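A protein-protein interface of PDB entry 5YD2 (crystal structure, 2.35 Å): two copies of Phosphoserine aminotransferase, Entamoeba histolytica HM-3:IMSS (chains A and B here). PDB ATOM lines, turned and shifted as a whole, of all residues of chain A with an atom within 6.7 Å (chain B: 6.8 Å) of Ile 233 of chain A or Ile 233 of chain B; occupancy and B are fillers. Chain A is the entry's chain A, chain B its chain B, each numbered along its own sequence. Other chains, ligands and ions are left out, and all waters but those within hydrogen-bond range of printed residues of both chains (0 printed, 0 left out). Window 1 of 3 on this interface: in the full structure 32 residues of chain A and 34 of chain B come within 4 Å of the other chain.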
ATOM      1  N   THR A  20      -1.308 -12.557  -3.665  1.00  0.00           N
ATOM      2  CA  THR A  20      -1.240 -14.004  -3.816  1.00  0.00           C
ATOM      3  C   THR A  20      -1.597 -14.437  -5.233  1.00  0.00           C
ATOM      4  O   THR A  20      -0.906 -15.279  -5.813  1.00  0.00           O
ATOM      5  CB  THR A  20      -2.173 -14.726  -2.828  1.00  0.00           C
ATOM      6  OG1 THR A  20      -1.778 -14.426  -1.491  1.00  0.00           O
ATOM      7  CG2 THR A  20      -2.125 -16.217  -3.012  1.00  0.00           C
ATOM      8  N   ALA A  23       1.117 -13.598  -7.555  1.00  0.00           N
ATOM      9  CA  ALA A  23       2.234 -14.529  -7.366  1.00  0.00           C
ATOM     10  C   ALA A  23       1.987 -15.925  -7.978  1.00  0.00           C
ATOM     11  O   ALA A  23       2.945 -16.626  -8.317  1.00  0.00           O
ATOM     12  CB  ALA A  23       2.591 -14.645  -5.893  1.00  0.00           C
ATOM     13  N   VAL A  24       0.724 -16.317  -8.125  1.00  0.00           N
ATOM     14  CA  VAL A  24       0.362 -17.564  -8.807  1.00  0.00           C
ATOM     15  C   VAL A  24       0.525 -17.476 -10.316  1.00  0.00           C
ATOM     16  O   VAL A  24       0.916 -18.448 -10.962  1.00  0.00           O
ATOM     17  CB  VAL A  24      -1.097 -17.956  -8.503  1.00  0.00           C
ATOM     18  CG1 VAL A  24      -1.606 -19.049  -9.436  1.00  0.00           C
ATOM     19  CG2 VAL A  24      -1.217 -18.414  -7.058  1.00  0.00           C
ATOM     20  N   ILE A  33       4.470 -19.102  -8.505  1.00  0.00           N
ATOM     21  CA  ILE A  33       4.858 -19.547  -7.190  1.00  0.00           C
ATOM     22  C   ILE A  33       4.556 -21.038  -6.954  1.00  0.00           C
ATOM     23  O   ILE A  33       5.169 -21.650  -6.101  1.00  0.00           O
ATOM     24  CB  ILE A  33       4.256 -18.680  -6.055  1.00  0.00           C
ATOM     25  CG1 ILE A  33       4.878 -19.095  -4.710  1.00  0.00           C
ATOM     26  CG2 ILE A  33       2.741 -18.804  -5.994  1.00  0.00           C
ATOM     27  CD1 ILE A  33       4.893 -17.993  -3.692  1.00  0.00           C
ATOM     28  N   LEU A  34       3.600 -21.611  -7.679  1.00  0.00           N
ATOM     29  CA  LEU A  34       3.265 -23.028  -7.513  1.00  0.00           C
ATOM     30  C   LEU A  34       4.307 -23.929  -8.132  1.00  0.00           C
ATOM     31  O   LEU A  34       4.264 -25.136  -7.920  1.00  0.00           O
ATOM     32  CB  LEU A  34       1.906 -23.373  -8.157  1.00  0.00           C
ATOM     33  CG  LEU A  34       0.703 -22.493  -7.796  1.00  0.00           C
ATOM     34  CD1 LEU A  34      -0.563 -22.880  -8.540  1.00  0.00           C
ATOM     35  CD2 LEU A  34       0.458 -22.517  -6.296  1.00  0.00           C
ATOM     36  N   TRP A  43      12.903 -18.541  -3.091  1.00  0.00           N
ATOM     37  CA  TRP A  43      12.047 -18.985  -2.029  1.00  0.00           C
ATOM     38  C   TRP A  43      12.662 -18.812  -0.645  1.00  0.00           C
ATOM     39  O   TRP A  43      11.981 -18.381   0.287  1.00  0.00           O
ATOM     40  CB  TRP A  43      11.604 -20.442  -2.217  1.00  0.00           C
ATOM     41  CG  TRP A  43      10.662 -20.759  -1.116  1.00  0.00           C
ATOM     42  CD1 TRP A  43      10.837 -21.670  -0.107  1.00  0.00           C
ATOM     43  CD2 TRP A  43       9.447 -20.065  -0.825  1.00  0.00           C
ATOM     44  NE1 TRP A  43       9.787 -21.591   0.791  1.00  0.00           N
ATOM     45  CE2 TRP A  43       8.910 -20.635   0.348  1.00  0.00           C
ATOM     46  CE3 TRP A  43       8.745 -19.039  -1.458  1.00  0.00           C
ATOM     47  CZ2 TRP A  43       7.696 -20.212   0.899  1.00  0.00           C
ATOM     48  CZ3 TRP A  43       7.565 -18.608  -0.893  1.00  0.00           C
ATOM     49  CH2 TRP A  43       7.051 -19.206   0.269  1.00  0.00           C
ATOM     50  N   ALA A 191      -3.670 -18.240   5.324  1.00  0.00           N
ATOM     51  CA  ALA A 191      -4.573 -19.139   4.712  1.00  0.00           C
ATOM     52  C   ALA A 191      -4.298 -20.568   5.156  1.00  0.00           C
ATOM     53  O   ALA A 191      -3.197 -20.915   5.558  1.00  0.00           O
ATOM     54  CB  ALA A 191      -4.477 -19.025   3.210  1.00  0.00           C
ATOM     55  N   ALA A 192      -5.345 -21.384   5.089  1.00  0.00           N
ATOM     56  CA  ALA A 192      -5.323 -22.753   5.535  1.00  0.00           C
ATOM     57  C   ALA A 192      -4.184 -23.503   4.868  1.00  0.00           C
ATOM     58  O   ALA A 192      -3.925 -23.316   3.680  1.00  0.00           O
ATOM     59  CB  ALA A 192      -6.638 -23.428   5.185  1.00  0.00           C
ATOM     60  N   GLY A 193      -3.507 -24.319   5.663  1.00  0.00           N
ATOM     61  CA  GLY A 193      -2.372 -25.107   5.219  1.00  0.00           C
ATOM     62  C   GLY A 193      -1.090 -24.844   5.973  1.00  0.00           C
ATOM     63  O   GLY A 193      -0.127 -25.574   5.768  1.00  0.00           O
ATOM     64  N   PRO A 230       7.944 -27.369   2.640  1.00  0.00           N
ATOM     65  CA  PRO A 230       7.024 -26.571   3.405  1.00  0.00           C
ATOM     66  C   PRO A 230       5.834 -26.167   2.554  1.00  0.00           C
ATOM     67  O   PRO A 230       5.903 -26.259   1.323  1.00  0.00           O
ATOM     68  CB  PRO A 230       7.864 -25.346   3.764  1.00  0.00           C
ATOM     69  CG  PRO A 230       8.858 -25.193   2.632  1.00  0.00           C
ATOM     70  CD  PRO A 230       8.985 -26.536   1.972  1.00  0.00           C
ATOM     71  N   PRO A 231       4.763 -25.684   3.197  1.00  0.00           N
ATOM     72  CA  PRO A 231       3.563 -25.223   2.505  1.00  0.00           C
ATOM     73  C   PRO A 231       3.707 -23.813   1.880  1.00  0.00           C
ATOM     74  O   PRO A 231       3.187 -22.817   2.432  1.00  0.00           O
ATOM     75  CB  PRO A 231       2.498 -25.268   3.627  1.00  0.00           C
ATOM     76  CG  PRO A 231       3.271 -24.977   4.873  1.00  0.00           C
ATOM     77  CD  PRO A 231       4.616 -25.613   4.669  1.00  0.00           C
ATOM     78  N   VAL A 232       4.336 -23.763   0.703  1.00  0.00           N
ATOM     79  CA  VAL A 232       4.865 -22.528   0.101  1.00  0.00           C
ATOM     80  C   VAL A 232       3.829 -21.405  -0.044  1.00  0.00           C
ATOM     81  O   VAL A 232       4.019 -20.263   0.436  1.00  0.00           O
ATOM     82  CB  VAL A 232       5.541 -22.848  -1.275  1.00  0.00           C
ATOM     83  CG1 VAL A 232       5.743 -21.614  -2.155  1.00  0.00           C
ATOM     84  CG2 VAL A 232       6.871 -23.525  -1.044  1.00  0.00           C
ATOM     85  N   ILE A 233       2.725 -21.732  -0.690  1.00  0.00           N
ATOM     86  CA  ILE A 233       1.721 -20.731  -0.957  1.00  0.00           C
ATOM     87  C   ILE A 233       1.062 -20.176   0.301  1.00  0.00           C
ATOM     88  O   ILE A 233       0.862 -18.960   0.420  1.00  0.00           O
ATOM     89  CB  ILE A 233       0.671 -21.260  -1.944  1.00  0.00           C
ATOM     90  CG1 ILE A 233      -0.171 -20.098  -2.468  1.00  0.00           C
ATOM     91  CG2 ILE A 233      -0.179 -22.353  -1.309  1.00  0.00           C
ATOM     92  CD1 ILE A 233      -0.475 -20.246  -3.935  1.00  0.00           C
ATOM     93  N   SER A 234       0.762 -21.043   1.259  1.00  0.00           N
ATOM     94  CA  SER A 234       0.188 -20.575   2.531  1.00  0.00           C
ATOM     95  C   SER A 234       1.180 -19.663   3.269  1.00  0.00           C
ATOM     96  O   SER A 234       0.780 -18.690   3.931  1.00  0.00           O
ATOM     97  CB  SER A 234      -0.241 -21.768   3.395  1.00  0.00           C
ATOM     98  OG  SER A 234      -1.310 -22.502   2.766  1.00  0.00           O
ATOM     99  N   ILE A 235       2.474 -19.969   3.142  1.00  0.00           N
ATOM    100  CA  ILE A 235       3.516 -19.174   3.768  1.00  0.00           C
ATOM    101  C   ILE A 235       3.599 -17.828   3.089  1.00  0.00           C
ATOM    102  O   ILE A 235       3.723 -16.787   3.757  1.00  0.00           O
ATOM    103  CB  ILE A 235       4.893 -19.864   3.698  1.00  0.00           C
ATOM    104  CG1 ILE A 235       4.941 -21.024   4.681  1.00  0.00           C
ATOM    105  CG2 ILE A 235       5.987 -18.875   4.037  1.00  0.00           C
ATOM    106  CD1 ILE A 235       6.050 -21.989   4.441  1.00  0.00           C
ATOM    107  N   PHE A 236       3.513 -17.827   1.765  1.00  0.00           N
ATOM    108  CA  PHE A 236       3.423 -16.565   1.057  1.00  0.00           C
ATOM    109  C   PHE A 236       2.261 -15.660   1.562  1.00  0.00           C
ATOM    110  O   PHE A 236       2.443 -14.442   1.756  1.00  0.00           O
ATOM    111  CB  PHE A 236       3.249 -16.811  -0.430  1.00  0.00           C
ATOM    112  CG  PHE A 236       3.361 -15.566  -1.242  1.00  0.00           C
ATOM    113  CD1 PHE A 236       4.615 -15.008  -1.516  1.00  0.00           C
ATOM    114  CD2 PHE A 236       2.230 -14.938  -1.726  1.00  0.00           C
ATOM    115  CE1 PHE A 236       4.729 -13.836  -2.263  1.00  0.00           C
ATOM    116  CE2 PHE A 236       2.335 -13.780  -2.489  1.00  0.00           C
ATOM    117  CZ  PHE A 236       3.574 -13.225  -2.750  1.00  0.00           C
ATOM    118  N   THR A 237       1.075 -16.240   1.786  1.00  0.00           N
ATOM    119  CA  THR A 237      -0.064 -15.431   2.223  1.00  0.00           C
ATOM    120  C   THR A 237       0.224 -14.814   3.591  1.00  0.00           C
ATOM    121  O   THR A 237      -0.180 -13.679   3.865  1.00  0.00           O
ATOM    122  CB  THR A 237      -1.378 -16.236   2.305  1.00  0.00           C
ATOM    123  OG1 THR A 237      -1.325 -17.150   3.394  1.00  0.00           O
ATOM    124  CG2 THR A 237      -1.648 -16.993   1.022  1.00  0.00           C
ATOM    125  N   VAL A 238       0.925 -15.554   4.444  1.00  0.00           N
ATOM    126  CA  VAL A 238       1.381 -14.992   5.725  1.00  0.00           C
ATOM    127  C   VAL A 238       2.352 -13.842   5.507  1.00  0.00           C
ATOM    128  O   VAL A 238       2.339 -12.839   6.235  1.00  0.00           O
ATOM    129  CB  VAL A 238       2.085 -16.068   6.563  1.00  0.00           C
ATOM    130  CG1 VAL A 238       2.871 -15.473   7.726  1.00  0.00           C
ATOM    131  CG2 VAL A 238       1.067 -17.084   7.035  1.00  0.00           C
ATOM    132  N   THR B  20      -6.196 -22.117 -10.546  1.00  0.00           N
ATOM    133  CA  THR B  20      -5.854 -21.781  -9.181  1.00  0.00           C
ATOM    134  C   THR B  20      -5.890 -20.281  -8.959  1.00  0.00           C
ATOM    135  O   THR B  20      -6.426 -19.828  -7.961  1.00  0.00           O
ATOM    136  CB  THR B  20      -4.473 -22.335  -8.777  1.00  0.00           C
ATOM    137  OG1 THR B  20      -4.499 -23.768  -8.839  1.00  0.00           O
ATOM    138  CG2 THR B  20      -4.134 -21.937  -7.351  1.00  0.00           C
ATOM    139  N   ALA B  23      -9.333 -19.099  -8.844  1.00  0.00           N
ATOM    140  CA  ALA B  23      -9.988 -19.499  -7.603  1.00  0.00           C
ATOM    141  C   ALA B  23      -9.591 -18.641  -6.413  1.00  0.00           C
ATOM    142  O   ALA B  23     -10.354 -18.503  -5.457  1.00  0.00           O
ATOM    143  CB  ALA B  23      -9.756 -20.973  -7.324  1.00  0.00           C
ATOM    144  N   VAL B  24      -8.396 -18.060  -6.475  1.00  0.00           N
ATOM    145  CA  VAL B  24      -7.952 -17.102  -5.467  1.00  0.00           C
ATOM    146  C   VAL B  24      -8.689 -15.761  -5.569  1.00  0.00           C
ATOM    147  O   VAL B  24      -8.945 -15.110  -4.552  1.00  0.00           O
ATOM    148  CB  VAL B  24      -6.425 -16.864  -5.581  1.00  0.00           C
ATOM    149  CG1 VAL B  24      -5.969 -15.656  -4.769  1.00  0.00           C
ATOM    150  CG2 VAL B  24      -5.684 -18.096  -5.115  1.00  0.00           C
ATOM    151  N   ILE B  33     -11.008 -18.393  -2.614  1.00  0.00           N
ATOM    152  CA  ILE B  33     -10.766 -19.694  -2.017  1.00  0.00           C
ATOM    153  C   ILE B  33      -9.955 -19.597  -0.727  1.00  0.00           C
ATOM    154  O   ILE B  33     -10.072 -20.466   0.134  1.00  0.00           O
ATOM    155  CB  ILE B  33     -10.123 -20.689  -2.976  1.00  0.00           C
ATOM    156  CG1 ILE B  33     -10.105 -22.073  -2.321  1.00  0.00           C
ATOM    157  CG2 ILE B  33      -8.724 -20.261  -3.369  1.00  0.00           C
ATOM    158  CD1 ILE B  33     -10.118 -23.216  -3.303  1.00  0.00           C
ATOM    159  N   LEU B  34      -9.199 -18.514  -0.541  1.00  0.00           N
ATOM    160  CA  LEU B  34      -8.473 -18.310   0.720  1.00  0.00           C
ATOM    161  C   LEU B  34      -9.386 -17.902   1.897  1.00  0.00           C
ATOM    162  O   LEU B  34      -8.915 -17.867   3.040  1.00  0.00           O
ATOM    163  CB  LEU B  34      -7.372 -17.240   0.561  1.00  0.00           C
ATOM    164  CG  LEU B  34      -6.436 -17.360  -0.664  1.00  0.00           C
ATOM    165  CD1 LEU B  34      -5.456 -16.213  -0.770  1.00  0.00           C
ATOM    166  CD2 LEU B  34      -5.699 -18.698  -0.665  1.00  0.00           C
ATOM    167  N   TRP B  43     -16.909 -26.184   0.005  1.00  0.00           N
ATOM    168  CA  TRP B  43     -15.649 -26.853   0.176  1.00  0.00           C
ATOM    169  C   TRP B  43     -15.789 -28.364   0.302  1.00  0.00           C
ATOM    170  O   TRP B  43     -14.990 -29.106  -0.296  1.00  0.00           O
ATOM    171  CB  TRP B  43     -14.855 -26.314   1.363  1.00  0.00           C
ATOM    172  CG  TRP B  43     -13.546 -27.027   1.377  1.00  0.00           C
ATOM    173  CD1 TRP B  43     -13.084 -27.891   2.315  1.00  0.00           C
ATOM    174  CD2 TRP B  43     -12.577 -27.029   0.322  1.00  0.00           C
ATOM    175  NE1 TRP B  43     -11.874 -28.404   1.925  1.00  0.00           N
ATOM    176  CE2 TRP B  43     -11.554 -27.901   0.697  1.00  0.00           C
ATOM    177  CE3 TRP B  43     -12.489 -26.375  -0.916  1.00  0.00           C
ATOM    178  CZ2 TRP B  43     -10.446 -28.108  -0.084  1.00  0.00           C
ATOM    179  CZ3 TRP B  43     -11.365 -26.586  -1.707  1.00  0.00           C
ATOM    180  CH2 TRP B  43     -10.364 -27.441  -1.284  1.00  0.00           C
ATOM    181  N   ALA B 191       0.550 -29.040  -5.550  1.00  0.00           N
ATOM    182  CA  ALA B 191       1.457 -28.041  -5.058  1.00  0.00           C
ATOM    183  C   ALA B 191       1.789 -28.349  -3.617  1.00  0.00           C
ATOM    184  O   ALA B 191       1.036 -29.031  -2.903  1.00  0.00           O
ATOM    185  CB  ALA B 191       0.826 -26.673  -5.185  1.00  0.00           C
ATOM    186  N   ALA B 192       2.901 -27.795  -3.182  1.00  0.00           N
ATOM    187  CA  ALA B 192       3.401 -28.007  -1.856  1.00  0.00           C
ATOM    188  C   ALA B 192       2.347 -27.649  -0.843  1.00  0.00           C
ATOM    189  O   ALA B 192       1.664 -26.640  -0.969  1.00  0.00           O
ATOM    190  CB  ALA B 192       4.625 -27.137  -1.637  1.00  0.00           C
ATOM    191  N   GLY B 193       2.257 -28.477   0.187  1.00  0.00           N
ATOM    192  CA  GLY B 193       1.343 -28.277   1.299  1.00  0.00           C
ATOM    193  C   GLY B 193       0.359 -29.405   1.508  1.00  0.00           C
ATOM    194  O   GLY B 193      -0.311 -29.419   2.549  1.00  0.00           O
ATOM    195  N   PRO B 230      -7.942 -28.627   6.806  1.00  0.00           N
ATOM    196  CA  PRO B 230      -7.108 -29.233   5.784  1.00  0.00           C
ATOM    197  C   PRO B 230      -6.497 -28.153   4.916  1.00  0.00           C
ATOM    198  O   PRO B 230      -6.933 -26.990   4.998  1.00  0.00           O
ATOM    199  CB  PRO B 230      -8.114 -30.048   4.953  1.00  0.00           C
ATOM    200  CG  PRO B 230      -9.394 -29.296   5.078  1.00  0.00           C
ATOM    201  CD  PRO B 230      -9.328 -28.476   6.332  1.00  0.00           C
ATOM    202  N   PRO B 231      -5.526 -28.531   4.074  1.00  0.00           N
ATOM    203  CA  PRO B 231      -4.786 -27.572   3.272  1.00  0.00           C
ATOM    204  C   PRO B 231      -5.494 -27.240   1.976  1.00  0.00           C
ATOM    205  O   PRO B 231      -5.150 -27.750   0.915  1.00  0.00           O
ATOM    206  CB  PRO B 231      -3.430 -28.296   3.038  1.00  0.00           C
ATOM    207  CG  PRO B 231      -3.768 -29.743   3.087  1.00  0.00           C
ATOM    208  CD  PRO B 231      -4.850 -29.859   4.108  1.00  0.00           C
ATOM    209  N   VAL B 232      -6.418 -26.299   2.074  1.00  0.00           N
ATOM    210  CA  VAL B 232      -7.461 -26.088   1.073  1.00  0.00           C
ATOM    211  C   VAL B 232      -6.917 -25.820  -0.305  1.00  0.00           C
ATOM    212  O   VAL B 232      -7.290 -26.497  -1.279  1.00  0.00           O
ATOM    213  CB  VAL B 232      -8.446 -24.947   1.545  1.00  0.00           C
ATOM    214  CG1 VAL B 232      -9.279 -24.370   0.422  1.00  0.00           C
ATOM    215  CG2 VAL B 232      -9.351 -25.464   2.650  1.00  0.00           C
ATOM    216  N   ILE B 233      -6.045 -24.829  -0.397  1.00  0.00           N
ATOM    217  CA  ILE B 233      -5.568 -24.392  -1.688  1.00  0.00           C
ATOM    218  C   ILE B 233      -4.734 -25.461  -2.361  1.00  0.00           C
ATOM    219  O   ILE B 233      -4.878 -25.711  -3.564  1.00  0.00           O
ATOM    220  CB  ILE B 233      -4.814 -23.064  -1.589  1.00  0.00           C
ATOM    221  CG1 ILE B 233      -4.584 -22.490  -2.988  1.00  0.00           C
ATOM    222  CG2 ILE B 233      -3.496 -23.224  -0.837  1.00  0.00           C
ATOM    223  CD1 ILE B 233      -4.742 -20.994  -3.016  1.00  0.00           C
ATOM    224  N   SER B 234      -3.893 -26.141  -1.600  1.00  0.00           N
ATOM    225  CA  SER B 234      -3.104 -27.255  -2.179  1.00  0.00           C
ATOM    226  C   SER B 234      -4.008 -28.407  -2.640  1.00  0.00           C
ATOM    227  O   SER B 234      -3.740 -29.023  -3.669  1.00  0.00           O
ATOM    228  CB  SER B 234      -2.100 -27.767  -1.170  1.00  0.00           C
ATOM    229  OG  SER B 234      -1.164 -26.750  -0.881  1.00  0.00           O
ATOM    230  N   ILE B 235      -5.101 -28.657  -1.913  1.00  0.00           N
ATOM    231  CA  ILE B 235      -6.059 -29.673  -2.299  1.00  0.00           C
ATOM    232  C   ILE B 235      -6.742 -29.248  -3.574  1.00  0.00           C
ATOM    233  O   ILE B 235      -6.983 -30.062  -4.470  1.00  0.00           O
ATOM    234  CB  ILE B 235      -7.131 -29.903  -1.199  1.00  0.00           C
ATOM    235  CG1 ILE B 235      -6.497 -30.673  -0.046  1.00  0.00           C
ATOM    236  CG2 ILE B 235      -8.302 -30.712  -1.745  1.00  0.00           C
ATOM    237  CD1 ILE B 235      -7.282 -30.634   1.218  1.00  0.00           C
ATOM    238  N   PHE B 236      -7.071 -27.966  -3.674  1.00  0.00           N
ATOM    239  CA  PHE B 236      -7.661 -27.461  -4.923  1.00  0.00           C
ATOM    240  C   PHE B 236      -6.763 -27.728  -6.138  1.00  0.00           C
ATOM    241  O   PHE B 236      -7.248 -28.155  -7.200  1.00  0.00           O
ATOM    242  CB  PHE B 236      -7.945 -25.974  -4.810  1.00  0.00           C
ATOM    243  CG  PHE B 236      -8.683 -25.433  -5.978  1.00  0.00           C
ATOM    244  CD1 PHE B 236     -10.055 -25.683  -6.117  1.00  0.00           C
ATOM    245  CD2 PHE B 236      -8.029 -24.707  -6.961  1.00  0.00           C
ATOM    246  CE1 PHE B 236     -10.750 -25.199  -7.211  1.00  0.00           C
ATOM    247  CE2 PHE B 236      -8.713 -24.226  -8.052  1.00  0.00           C
ATOM    248  CZ  PHE B 236     -10.076 -24.467  -8.179  1.00  0.00           C
ATOM    249  N   THR B 237      -5.455 -27.491  -5.993  1.00  0.00           N
ATOM    250  CA  THR B 237      -4.523 -27.672  -7.122  1.00  0.00           C
ATOM    251  C   THR B 237      -4.488 -29.128  -7.525  1.00  0.00           C
ATOM    252  O   THR B 237      -4.398 -29.429  -8.699  1.00  0.00           O
ATOM    253  CB  THR B 237      -3.081 -27.217  -6.812  1.00  0.00           C
ATOM    254  OG1 THR B 237      -2.480 -28.111  -5.866  1.00  0.00           O
ATOM    255  CG2 THR B 237      -3.042 -25.790  -6.257  1.00  0.00           C
ATOM    256  N   VAL B 238      -4.608 -30.030  -6.557  1.00  0.00           N
ATOM    257  CA  VAL B 238      -4.775 -31.464  -6.849  1.00  0.00           C
ATOM    258  C   VAL B 238      -6.054 -31.735  -7.600  1.00  0.00           C
ATOM    259  O   VAL B 238      -6.111 -32.562  -8.510  1.00  0.00           O
ATOM    260  CB  VAL B 238      -4.801 -32.301  -5.554  1.00  0.00           C
ATOM    261  CG1 VAL B 238      -5.278 -33.732  -5.790  1.00  0.00           C
ATOM    262  CG2 VAL B 238      -3.415 -32.289  -4.930  1.00  0.00           C
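Of the 18 printed residues of chain B, 6 touch a printed residue of chain A. Hydrophobic or aromatic side chains of chain B that line the printed part of chain A: Ala 192 and Ile 233.
Among the printed residues, merely in contact across the chains: Leu 34 of chain A with Thr 20 of chain B (3.9 Å), Ala 192 of chain A with Pro 230 of chain B (3.6 Å), Gly 193 of chain A with Pro 231 of chain B (3.96 Å), Pro 230 of chain A with Ala 192 of chain B (3.3 Å), Pro 231 of chain A with Gly 193 of chain B (3.96 Å) and Ile 233 of chain A with Ile 233 of chain B (3.5 Å).
Of chain B, only Ile 233 comes within 4 Å of Ile 233 of chain A. Of chain A, only Ile 233 comes within 4 Å of Ile 233 of chain B. Printed residues of chain B within 4 Å of Pro 231 of chain A: Gly 193. Printed residues of chain A within 4 Å of Pro 230 of chain B: Ala 192. Val 232 of chain A touches none of the printed residues of chain B. The nearest residue of chain A that does not touch Ile 233 of chain B is Ser 234 of chain A (4.3 Å). The nearest printed residue of chain B that does not touch Pro 230 of chain A is Gly 193 of chain B (4.4 Å).
The backbone carbonyl oxygen (O) of Ala 192 of chain A sits at hydrogen-bond distance from the side-chain hydroxyl (OG) of Ser 234 of chain A (2.9 Å). OG of Ser 234 of chain B lies within hydrogen-bond range of O of Ala 192 of chain B, 2.8 Å away.
Leu 34 of chain A touches Thr 20 of chain B, but with the chains exchanged Thr 20 of chain A does not touch Leu 34 of chain B (4.02 Å). Ala 192 of chain A touches Pro 230 of chain B, and with the chains exchanged Pro 230 of chain A touches Ala 192 of chain B. Gly 193 of chain A touches Pro 231 of chain B, and with the chains exchanged Pro 231 of chain A touches Gly 193 of chain B. Ile 233 of chain B touches its own counterpart, Ile 233 of chain A. Positions printed for both chains: 20, 23, 24, 33, 34, 43, 191, 192, 193, 230, 231, 232, 233, 234, 235, 236, 237 and 238. Of the 6 pairs that touch across the chains among the printed residues, 5 have their exchanged pair printed and touching as well.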
